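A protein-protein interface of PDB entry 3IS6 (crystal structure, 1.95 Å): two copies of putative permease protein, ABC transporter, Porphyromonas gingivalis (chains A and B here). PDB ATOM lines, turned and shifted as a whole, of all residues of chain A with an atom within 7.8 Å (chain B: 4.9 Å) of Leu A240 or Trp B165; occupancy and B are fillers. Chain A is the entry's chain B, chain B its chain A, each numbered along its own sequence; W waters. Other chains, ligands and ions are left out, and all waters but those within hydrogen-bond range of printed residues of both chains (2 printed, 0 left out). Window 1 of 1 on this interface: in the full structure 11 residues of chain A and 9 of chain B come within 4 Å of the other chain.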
ATOM      1  N   TYR A  63      12.624  16.354  26.075  1.00  0.00           N
ATOM      2  CA  TYR A  63      13.254  16.998  24.934  1.00  0.00           C
ATOM      3  C   TYR A  63      14.751  17.148  25.001  1.00  0.00           C
ATOM      4  O   TYR A  63      15.434  16.877  24.074  1.00  0.00           O
ATOM      5  CB  TYR A  63      12.612  18.306  24.537  1.00  0.00           C
ATOM      6  CG  TYR A  63      13.270  18.889  23.331  1.00  0.00           C
ATOM      7  CD1 TYR A  63      13.010  18.407  22.088  1.00  0.00           C
ATOM      8  CD2 TYR A  63      14.199  19.882  23.453  1.00  0.00           C
ATOM      9  CE1 TYR A  63      13.629  18.908  21.014  1.00  0.00           C
ATOM     10  CE2 TYR A  63      14.823  20.386  22.394  1.00  0.00           C
ATOM     11  CZ  TYR A  63      14.544  19.903  21.162  1.00  0.00           C
ATOM     12  OH  TYR A  63      15.166  20.428  20.101  1.00  0.00           O
ATOM     13  N   PRO A 234      21.505   5.109  30.678  1.00  0.00           N
ATOM     14  CA  PRO A 234      21.063   5.547  29.366  1.00  0.00           C
ATOM     15  C   PRO A 234      21.420   4.619  28.268  1.00  0.00           C
ATOM     16  O   PRO A 234      22.526   4.224  28.189  1.00  0.00           O
ATOM     17  CB  PRO A 234      21.834   6.822  29.184  1.00  0.00           C
ATOM     18  CG  PRO A 234      22.981   6.647  29.959  1.00  0.00           C
ATOM     19  CD  PRO A 234      22.596   5.940  31.169  1.00  0.00           C
ATOM     20  N   THR A 235      20.462   4.289  27.431  1.00  0.00           N
ATOM     21  CA  THR A 235      20.735   3.626  26.199  1.00  0.00           C
ATOM     22  C   THR A 235      21.200   4.623  25.137  1.00  0.00           C
ATOM     23  O   THR A 235      21.110   5.819  25.297  1.00  0.00           O
ATOM     24  CB  THR A 235      19.578   2.831  25.701  1.00  0.00           C
ATOM     25  OG1 THR A 235      18.583   3.714  25.241  1.00  0.00           O
ATOM     26  CG2 THR A 235      19.008   2.026  26.790  1.00  0.00           C
ATOM     27  N   LEU A 236      21.777   4.091  24.088  1.00  0.00           N
ATOM     28  CA  LEU A 236      22.294   4.897  23.032  1.00  0.00           C
ATOM     29  C   LEU A 236      21.198   5.626  22.297  1.00  0.00           C
ATOM     30  O   LEU A 236      21.360   6.750  21.956  1.00  0.00           O
ATOM     31  CB  LEU A 236      23.135   4.051  22.119  1.00  0.00           C
ATOM     32  CG  LEU A 236      24.193   4.826  21.393  1.00  0.00           C
ATOM     33  CD1 LEU A 236      25.278   3.937  20.906  1.00  0.00           C
ATOM     34  CD2 LEU A 236      23.465   5.393  20.279  1.00  0.00           C
ATOM     35  N   VAL A 237      20.074   4.966  22.069  1.00  0.00           N
ATOM     36  CA  VAL A 237      18.915   5.637  21.496  1.00  0.00           C
ATOM     37  C   VAL A 237      18.412   6.720  22.421  1.00  0.00           C
ATOM     38  O   VAL A 237      18.054   7.736  21.966  1.00  0.00           O
ATOM     39  CB  VAL A 237      17.737   4.721  21.178  1.00  0.00           C
ATOM     40  CG1 VAL A 237      17.828   4.178  19.807  1.00  0.00           C
ATOM     41  CG2 VAL A 237      17.589   3.650  22.201  1.00  0.00           C
ATOM     42  N   ASN A 238      18.397   6.501  23.717  1.00  0.00           N
ATOM     43  CA  ASN A 238      17.927   7.520  24.609  1.00  0.00           C
ATOM     44  C   ASN A 238      18.767   8.747  24.541  1.00  0.00           C
ATOM     45  O   ASN A 238      18.262   9.821  24.491  1.00  0.00           O
ATOM     46  CB  ASN A 238      18.084   7.060  26.040  1.00  0.00           C
ATOM     47  CG  ASN A 238      16.981   6.183  26.509  1.00  0.00           C
ATOM     48  OD1 ASN A 238      16.238   5.624  25.726  1.00  0.00           O
ATOM     49  ND2 ASN A 238      16.892   6.024  27.813  1.00  0.00           N
ATOM     50  N   MET A 239      20.074   8.580  24.590  1.00  0.00           N
ATOM     51  CA  MET A 239      20.977   9.699  24.494  1.00  0.00           C
ATOM     52  C   MET A 239      20.909  10.421  23.176  1.00  0.00           C
ATOM     53  O   MET A 239      20.968  11.613  23.132  1.00  0.00           O
ATOM     54  CB  MET A 239      22.395   9.274  24.747  1.00  0.00           C
ATOM     55  CG  MET A 239      22.596   8.639  26.065  1.00  0.00           C
ATOM     56  SD  MET A 239      24.421   8.399  26.502  1.00  0.00           S
ATOM     57  CE  MET A 239      24.691   6.610  26.044  1.00  0.00           C
ATOM     58  N   LEU A 240      20.798   9.670  22.104  1.00  0.00           N
ATOM     59  CA  LEU A 240      20.774  10.246  20.788  1.00  0.00           C
ATOM     60  C   LEU A 240      19.583  11.168  20.616  1.00  0.00           C
ATOM     61  O   LEU A 240      19.699  12.174  20.032  1.00  0.00           O
ATOM     62  CB  LEU A 240      20.780   9.171  19.722  1.00  0.00           C
ATOM     63  CG  LEU A 240      20.637   9.597  18.274  1.00  0.00           C
ATOM     64  CD1 LEU A 240      21.685  10.554  17.850  1.00  0.00           C
ATOM     65  CD2 LEU A 240      20.662   8.414  17.385  1.00  0.00           C
ATOM     66  N   ARG A 241      18.452  10.801  21.184  1.00  0.00           N
ATOM     67  CA  ARG A 241      17.238  11.573  21.045  1.00  0.00           C
ATOM     68  C   ARG A 241      17.335  12.971  21.590  1.00  0.00           C
ATOM     69  O   ARG A 241      16.694  13.826  21.095  1.00  0.00           O
ATOM     70  CB  ARG A 241      16.099  10.941  21.778  1.00  0.00           C
ATOM     71  CG  ARG A 241      15.764   9.595  21.399  1.00  0.00           C
ATOM     72  CD  ARG A 241      14.306   9.357  21.573  1.00  0.00           C
ATOM     73  NE  ARG A 241      14.009   7.980  21.338  1.00  0.00           N
ATOM     74  CZ  ARG A 241      14.177   7.052  22.238  1.00  0.00           C
ATOM     75  NH1 ARG A 241      14.629   7.382  23.413  1.00  0.00           N
ATOM     76  NH2 ARG A 241      13.888   5.817  21.962  1.00  0.00           N
ATOM     77  N   ILE A 242      18.096  13.184  22.649  1.00  0.00           N
ATOM     78  CA  ILE A 242      18.091  14.475  23.290  1.00  0.00           C
ATOM     79  C   ILE A 242      19.315  15.303  22.987  1.00  0.00           C
ATOM     80  O   ILE A 242      19.469  16.381  23.486  1.00  0.00           O
ATOM     81  CB  ILE A 242      17.907  14.365  24.802  1.00  0.00           C
ATOM     82  CG1 ILE A 242      19.097  13.708  25.430  1.00  0.00           C
ATOM     83  CG2 ILE A 242      16.745  13.532  25.145  1.00  0.00           C
ATOM     84  CD1 ILE A 242      19.041  13.747  26.886  1.00  0.00           C
ATOM     85  N   GLN A 243      20.175  14.790  22.135  1.00  0.00           N
ATOM     86  CA  GLN A 243      21.380  15.494  21.788  1.00  0.00           C
ATOM     87  C   GLN A 243      21.066  16.698  20.959  1.00  0.00           C
ATOM     88  O   GLN A 243      20.213  16.676  20.133  1.00  0.00           O
ATOM     89  CB  GLN A 243      22.326  14.600  21.010  1.00  0.00           C
ATOM     90  CG  GLN A 243      22.897  13.527  21.809  1.00  0.00           C
ATOM     91  CD  GLN A 243      23.503  14.062  23.055  1.00  0.00           C
ATOM     92  OE1 GLN A 243      24.359  14.911  23.010  1.00  0.00           O
ATOM     93  NE2 GLN A 243      23.033  13.593  24.171  1.00  0.00           N
ATOM     94  N   GLN A 244      21.801  17.756  21.195  1.00  0.00           N
ATOM     95  CA  GLN A 244      21.734  18.906  20.357  1.00  0.00           C
ATOM     96  C   GLN A 244      23.089  19.153  19.681  1.00  0.00           C
ATOM     97  O   GLN A 244      24.131  18.694  20.143  1.00  0.00           O
ATOM     98  CB  GLN A 244      21.296  20.102  21.171  1.00  0.00           C
ATOM     99  CG  GLN A 244      20.380  19.749  22.266  1.00  0.00           C
ATOM    100  CD  GLN A 244      18.999  19.546  21.792  1.00  0.00           C
ATOM    101  OE1 GLN A 244      18.437  20.418  21.213  1.00  0.00           O
ATOM    102  NE2 GLN A 244      18.433  18.395  22.050  1.00  0.00           N
ATOM    103  N   LEU B  82      32.772   6.437  24.740  1.00  0.00           N
ATOM    104  CA  LEU B  82      32.576   7.850  24.840  1.00  0.00           C
ATOM    105  C   LEU B  82      33.835   8.523  25.375  1.00  0.00           C
ATOM    106  O   LEU B  82      34.343   8.131  26.375  1.00  0.00           O
ATOM    107  CB  LEU B  82      31.403   8.126  25.746  1.00  0.00           C
ATOM    108  CG  LEU B  82      29.997   8.116  25.155  1.00  0.00           C
ATOM    109  CD1 LEU B  82      29.742   6.908  24.443  1.00  0.00           C
ATOM    110  CD2 LEU B  82      28.976   8.319  26.193  1.00  0.00           C
ATOM    111  N   ASN B 107      28.188  16.779  19.086  1.00  0.00           N
ATOM    112  CA  ASN B 107      27.458  15.645  19.585  1.00  0.00           C
ATOM    113  C   ASN B 107      26.832  14.803  18.497  1.00  0.00           C
ATOM    114  O   ASN B 107      26.560  13.668  18.706  1.00  0.00           O
ATOM    115  CB  ASN B 107      26.417  16.060  20.611  1.00  0.00           C
ATOM    116  CG  ASN B 107      27.022  16.446  21.948  1.00  0.00           C
ATOM    117  OD1 ASN B 107      27.827  15.740  22.502  1.00  0.00           O
ATOM    118  ND2 ASN B 107      26.618  17.566  22.462  1.00  0.00           N
ATOM    119  N   MET B 108      26.641  15.348  17.320  1.00  0.00           N
ATOM    120  CA  MET B 108      25.988  14.607  16.256  1.00  0.00           C
ATOM    121  C   MET B 108      26.961  13.910  15.306  1.00  0.00           C
ATOM    122  O   MET B 108      26.598  13.520  14.236  1.00  0.00           O
ATOM    123  CB  MET B 108      24.983  15.456  15.486  1.00  0.00           C
ATOM    124  CG  MET B 108      23.883  16.052  16.312  1.00  0.00           C
ATOM    125  SD  MET B 108      22.720  14.793  17.057  1.00  0.00           S
ATOM    126  CE  MET B 108      21.843  14.257  15.498  1.00  0.00           C
ATOM    127  N   PRO B 131      21.069   3.905  15.390  1.00  0.00           N
ATOM    128  CA  PRO B 131      20.904   2.664  16.111  1.00  0.00           C
ATOM    129  C   PRO B 131      19.918   1.831  15.370  1.00  0.00           C
ATOM    130  O   PRO B 131      18.994   2.324  14.820  1.00  0.00           O
ATOM    131  CB  PRO B 131      20.330   3.115  17.441  1.00  0.00           C
ATOM    132  CG  PRO B 131      20.685   4.453  17.556  1.00  0.00           C
ATOM    133  CD  PRO B 131      20.671   5.033  16.222  1.00  0.00           C
ATOM    134  N   ARG B 138      16.740  10.953  12.592  1.00  0.00           N
ATOM    135  CA  ARG B 138      17.929  11.515  13.191  1.00  0.00           C
ATOM    136  C   ARG B 138      19.075  10.523  13.071  1.00  0.00           C
ATOM    137  O   ARG B 138      18.908   9.358  13.258  1.00  0.00           O
ATOM    138  CB  ARG B 138      17.693  11.848  14.656  1.00  0.00           C
ATOM    139  CG  ARG B 138      18.919  12.170  15.417  1.00  0.00           C
ATOM    140  CD  ARG B 138      18.612  12.675  16.790  1.00  0.00           C
ATOM    141  NE  ARG B 138      18.139  14.028  16.706  1.00  0.00           N
ATOM    142  CZ  ARG B 138      18.346  14.974  17.593  1.00  0.00           C
ATOM    143  NH1 ARG B 138      19.034  14.754  18.681  1.00  0.00           N
ATOM    144  NH2 ARG B 138      17.862  16.156  17.362  1.00  0.00           N
ATOM    145  N   ILE B 140      23.681   9.968  13.183  1.00  0.00           N
ATOM    146  CA  ILE B 140      25.004  10.394  13.512  1.00  0.00           C
ATOM    147  C   ILE B 140      25.834  10.399  12.242  1.00  0.00           C
ATOM    148  O   ILE B 140      25.784   9.476  11.494  1.00  0.00           O
ATOM    149  CB  ILE B 140      25.638   9.443  14.495  1.00  0.00           C
ATOM    150  CG1 ILE B 140      24.761   9.284  15.720  1.00  0.00           C
ATOM    151  CG2 ILE B 140      26.930   9.942  14.914  1.00  0.00           C
ATOM    152  CD1 ILE B 140      24.990   8.000  16.453  1.00  0.00           C
ATOM    153  N   LEU B 161      32.374   8.452  20.430  1.00  0.00           N
ATOM    154  CA  LEU B 161      31.389   9.499  20.521  1.00  0.00           C
ATOM    155  C   LEU B 161      31.795  10.462  21.606  1.00  0.00           C
ATOM    156  O   LEU B 161      32.464  10.097  22.494  1.00  0.00           O
ATOM    157  CB  LEU B 161      30.044   8.922  20.870  1.00  0.00           C
ATOM    158  CG  LEU B 161      29.256   8.206  19.802  1.00  0.00           C
ATOM    159  CD1 LEU B 161      28.105   7.499  20.372  1.00  0.00           C
ATOM    160  CD2 LEU B 161      28.811   9.138  18.770  1.00  0.00           C
ATOM    161  N   PRO B 162      31.372  11.701  21.540  1.00  0.00           N
ATOM    162  CA  PRO B 162      31.762  12.631  22.576  1.00  0.00           C
ATOM    163  C   PRO B 162      31.165  12.295  23.925  1.00  0.00           C
ATOM    164  O   PRO B 162      30.048  11.890  24.034  1.00  0.00           O
ATOM    165  CB  PRO B 162      31.240  13.960  22.063  1.00  0.00           C
ATOM    166  CG  PRO B 162      30.975  13.769  20.733  1.00  0.00           C
ATOM    167  CD  PRO B 162      30.585  12.379  20.528  1.00  0.00           C
ATOM    168  N   ILE B 163      31.951  12.525  24.952  1.00  0.00           N
ATOM    169  CA  ILE B 163      31.575  12.252  26.308  1.00  0.00           C
ATOM    170  C   ILE B 163      30.402  13.095  26.742  1.00  0.00           C
ATOM    171  O   ILE B 163      29.675  12.724  27.592  1.00  0.00           O
ATOM    172  CB  ILE B 163      32.735  12.338  27.292  1.00  0.00           C
ATOM    173  CG1 ILE B 163      32.507  11.346  28.403  1.00  0.00           C
ATOM    174  CG2 ILE B 163      32.893  13.679  27.843  1.00  0.00           C
ATOM    175  CD1 ILE B 163      33.679  10.948  29.051  1.00  0.00           C
ATOM    176  N   THR B 164      30.194  14.191  26.036  1.00  0.00           N
ATOM    177  CA  THR B 164      29.128  15.140  26.292  1.00  0.00           C
ATOM    178  C   THR B 164      27.758  14.560  25.964  1.00  0.00           C
ATOM    179  O   THR B 164      26.784  15.161  26.204  1.00  0.00           O
ATOM    180  CB  THR B 164      29.325  16.476  25.576  1.00  0.00           C
ATOM    181  OG1 THR B 164      29.724  16.258  24.243  1.00  0.00           O
ATOM    182  CG2 THR B 164      30.357  17.270  26.248  1.00  0.00           C
ATOM    183  N   TRP B 165      27.714  13.385  25.402  1.00  0.00           N
ATOM    184  CA  TRP B 165      26.468  12.688  25.252  1.00  0.00           C
ATOM    185  C   TRP B 165      25.895  12.401  26.613  1.00  0.00           C
ATOM    186  O   TRP B 165      24.734  12.264  26.759  1.00  0.00           O
ATOM    187  CB  TRP B 165      26.636  11.390  24.502  1.00  0.00           C
ATOM    188  CG  TRP B 165      26.506  11.505  23.059  1.00  0.00           C
ATOM    189  CD1 TRP B 165      27.048  12.433  22.278  1.00  0.00           C
ATOM    190  CD2 TRP B 165      25.793  10.641  22.214  1.00  0.00           C
ATOM    191  NE1 TRP B 165      26.724  12.221  20.994  1.00  0.00           N
ATOM    192  CE2 TRP B 165      25.947  11.111  20.927  1.00  0.00           C
ATOM    193  CE3 TRP B 165      25.036   9.509  22.418  1.00  0.00           C
ATOM    194  CZ2 TRP B 165      25.371  10.508  19.863  1.00  0.00           C
ATOM    195  CZ3 TRP B 165      24.461   8.916  21.357  1.00  0.00           C
ATOM    196  CH2 TRP B 165      24.635   9.407  20.096  1.00  0.00           C
ATOM    197  N   MET B 166      26.745  12.262  27.598  1.00  0.00           N
ATOM    198  CA  MET B 166      26.301  11.968  28.937  1.00  0.00           C
ATOM    199  C   MET B 166      25.662  13.203  29.573  1.00  0.00           C
ATOM    200  O   MET B 166      26.067  14.290  29.327  1.00  0.00           O
ATOM    201  CB  MET B 166      27.452  11.451  29.808  1.00  0.00           C
ATOM    202  CG  MET B 166      28.059  10.145  29.392  1.00  0.00           C
ATOM    203  SD  MET B 166      27.002   8.621  29.750  1.00  0.00           S
ATOM    204  CE  MET B 166      27.018   8.676  31.557  1.00  0.00           C
ATOM    205  N   PRO B 167      24.702  12.993  30.431  1.00  0.00           N
ATOM    206  CA  PRO B 167      24.020  14.078  31.090  1.00  0.00           C
ATOM    207  C   PRO B 167      24.973  14.876  31.942  1.00  0.00           C
ATOM    208  O   PRO B 167      25.902  14.335  32.474  1.00  0.00           O
ATOM    209  CB  PRO B 167      23.068  13.339  31.990  1.00  0.00           C
ATOM    210  CG  PRO B 167      22.816  12.161  31.357  1.00  0.00           C
ATOM    211  CD  PRO B 167      24.010  11.738  30.663  1.00  0.00           C
HETATM  212  O   HOH W   1      27.211  19.588  20.071  1.00  0.00           O
HETATM  213  O   HOH W   2      16.347  17.516  19.249  1.00  0.00           O
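The backbone carbonyl oxygen (O) of Arg A241 is in hydrogen-bond range of the guanidinium group (NH1) of Arg B138. The backbone carbonyl oxygen (O) of Trp B165 is in hydrogen-bond range of the side-chain amide nitrogen (NE2) of Gln A243 (3.4 Å). The guanidinium group (NH1) of Arg B138 sits at hydrogen-bond distance from the backbone carbonyl oxygen (O) of Leu A240 (3.0 Å). The guanidinium group (NH1) of Arg B138 is in hydrogen-bond range of the backbone carbonyl oxygen (O) of Gln A243.
The backbone carbonyl oxygen (O) of Asn B107 sits at hydrogen-bond distance from the indole nitrogen (NE1) of Trp B165. The side-chain amide nitrogen (NE2) of Gln A243 lies close to the backbone carbonyl oxygen (O) of Met A239 (3.0 Å). The side-chain amide oxygen of Asn B107 sits at hydrogen-bond distance from the side-chain hydroxyl of Thr B164 (2.6 Å). OH of Tyr A63 is in hydrogen-bond range of OE1 of Gln A244 (3.5 Å). The backbone carbonyl oxygen (O) of Ile A242 sits at hydrogen-bond distance from the side-chain amide nitrogen (NE2) of Gln A244 (2.7 Å). NH1 of Arg A241 is in hydrogen-bond range of OD1 of Asn A238 (3.3 Å).
Among the printed residues, merely in contact across the chains: Leu A236 with Trp B165, Val A237 with Pro B131, Met A239 with Trp B165, Leu A240 with Pro B131, Leu A240 with Ile B140, Leu A240 with Trp B165, Gln A243 with Asn B107, Gln A243 with Met B108 and Gln A244 with Asn B107.
Of chain B, only Pro B131 (3.6 Å), Arg B138 (3.0 Å), Ile B140 (3.95 Å) and Trp B165 (3.8 Å) come within 4 Å of Leu A240. Of the printed residues of chain A, Asn B107 touches Gln A243 and Gln A244. Printed residues of chain B within 4 Å of Gln A243: Asn B107 (3.3 Å), Met B108 (3.98 Å), Arg B138 (2.7 Å) and Trp B165 (3.4 Å). Of the printed residues of chain B, Gln A244 touches Asn B107. Printed residues of chain B within 4 Å of Leu A236: Trp B165 (3.8 Å). Printed residues of chain A within 4 Å of Pro B131: Val A237 and Leu A240. Pro B162 touches none of the printed residues of chain A. Ile A242 touches none of the printed residues of chain B. The nearest residue of chain B that does not touch Leu A240 is Met B108 (4.4 Å). The nearest printed residue of chain A that does not touch Asn B107 is Leu A240 (5.8 Å).
Hydrophobic or aromatic side chains of chain A that line the printed part of chain B: Leu A236, Val A237, Met A239 and Leu A240. Along chain A the printed residues that touch a printed residue of chain B span positions 236 to 244. Of the 13 printed residues of chain B, 6 touch a printed residue of chain A. Printed residues of chain B that touch a printed residue of chain A: Asn B107, Met B108, Pro B131, Arg B138, Ile B140 and Trp B165. Among the printed residues, 13 pairs touch across the chains. Among the printed residues, no Asp or Glu carboxylate lies within 4 Å of a Lys or Arg side-chain nitrogen of the other chain.
No position is printed for both chains. Of the 13 pairs that touch across the chains among the printed residues, none has its exchanged pair printed and touching as well.
Water W2 bridges NH2 of Arg B138 and OH of Tyr A63. Water W1 bridges N of Asn B107 (3.1 Å) and O of Gln A244 (3.2 Å).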
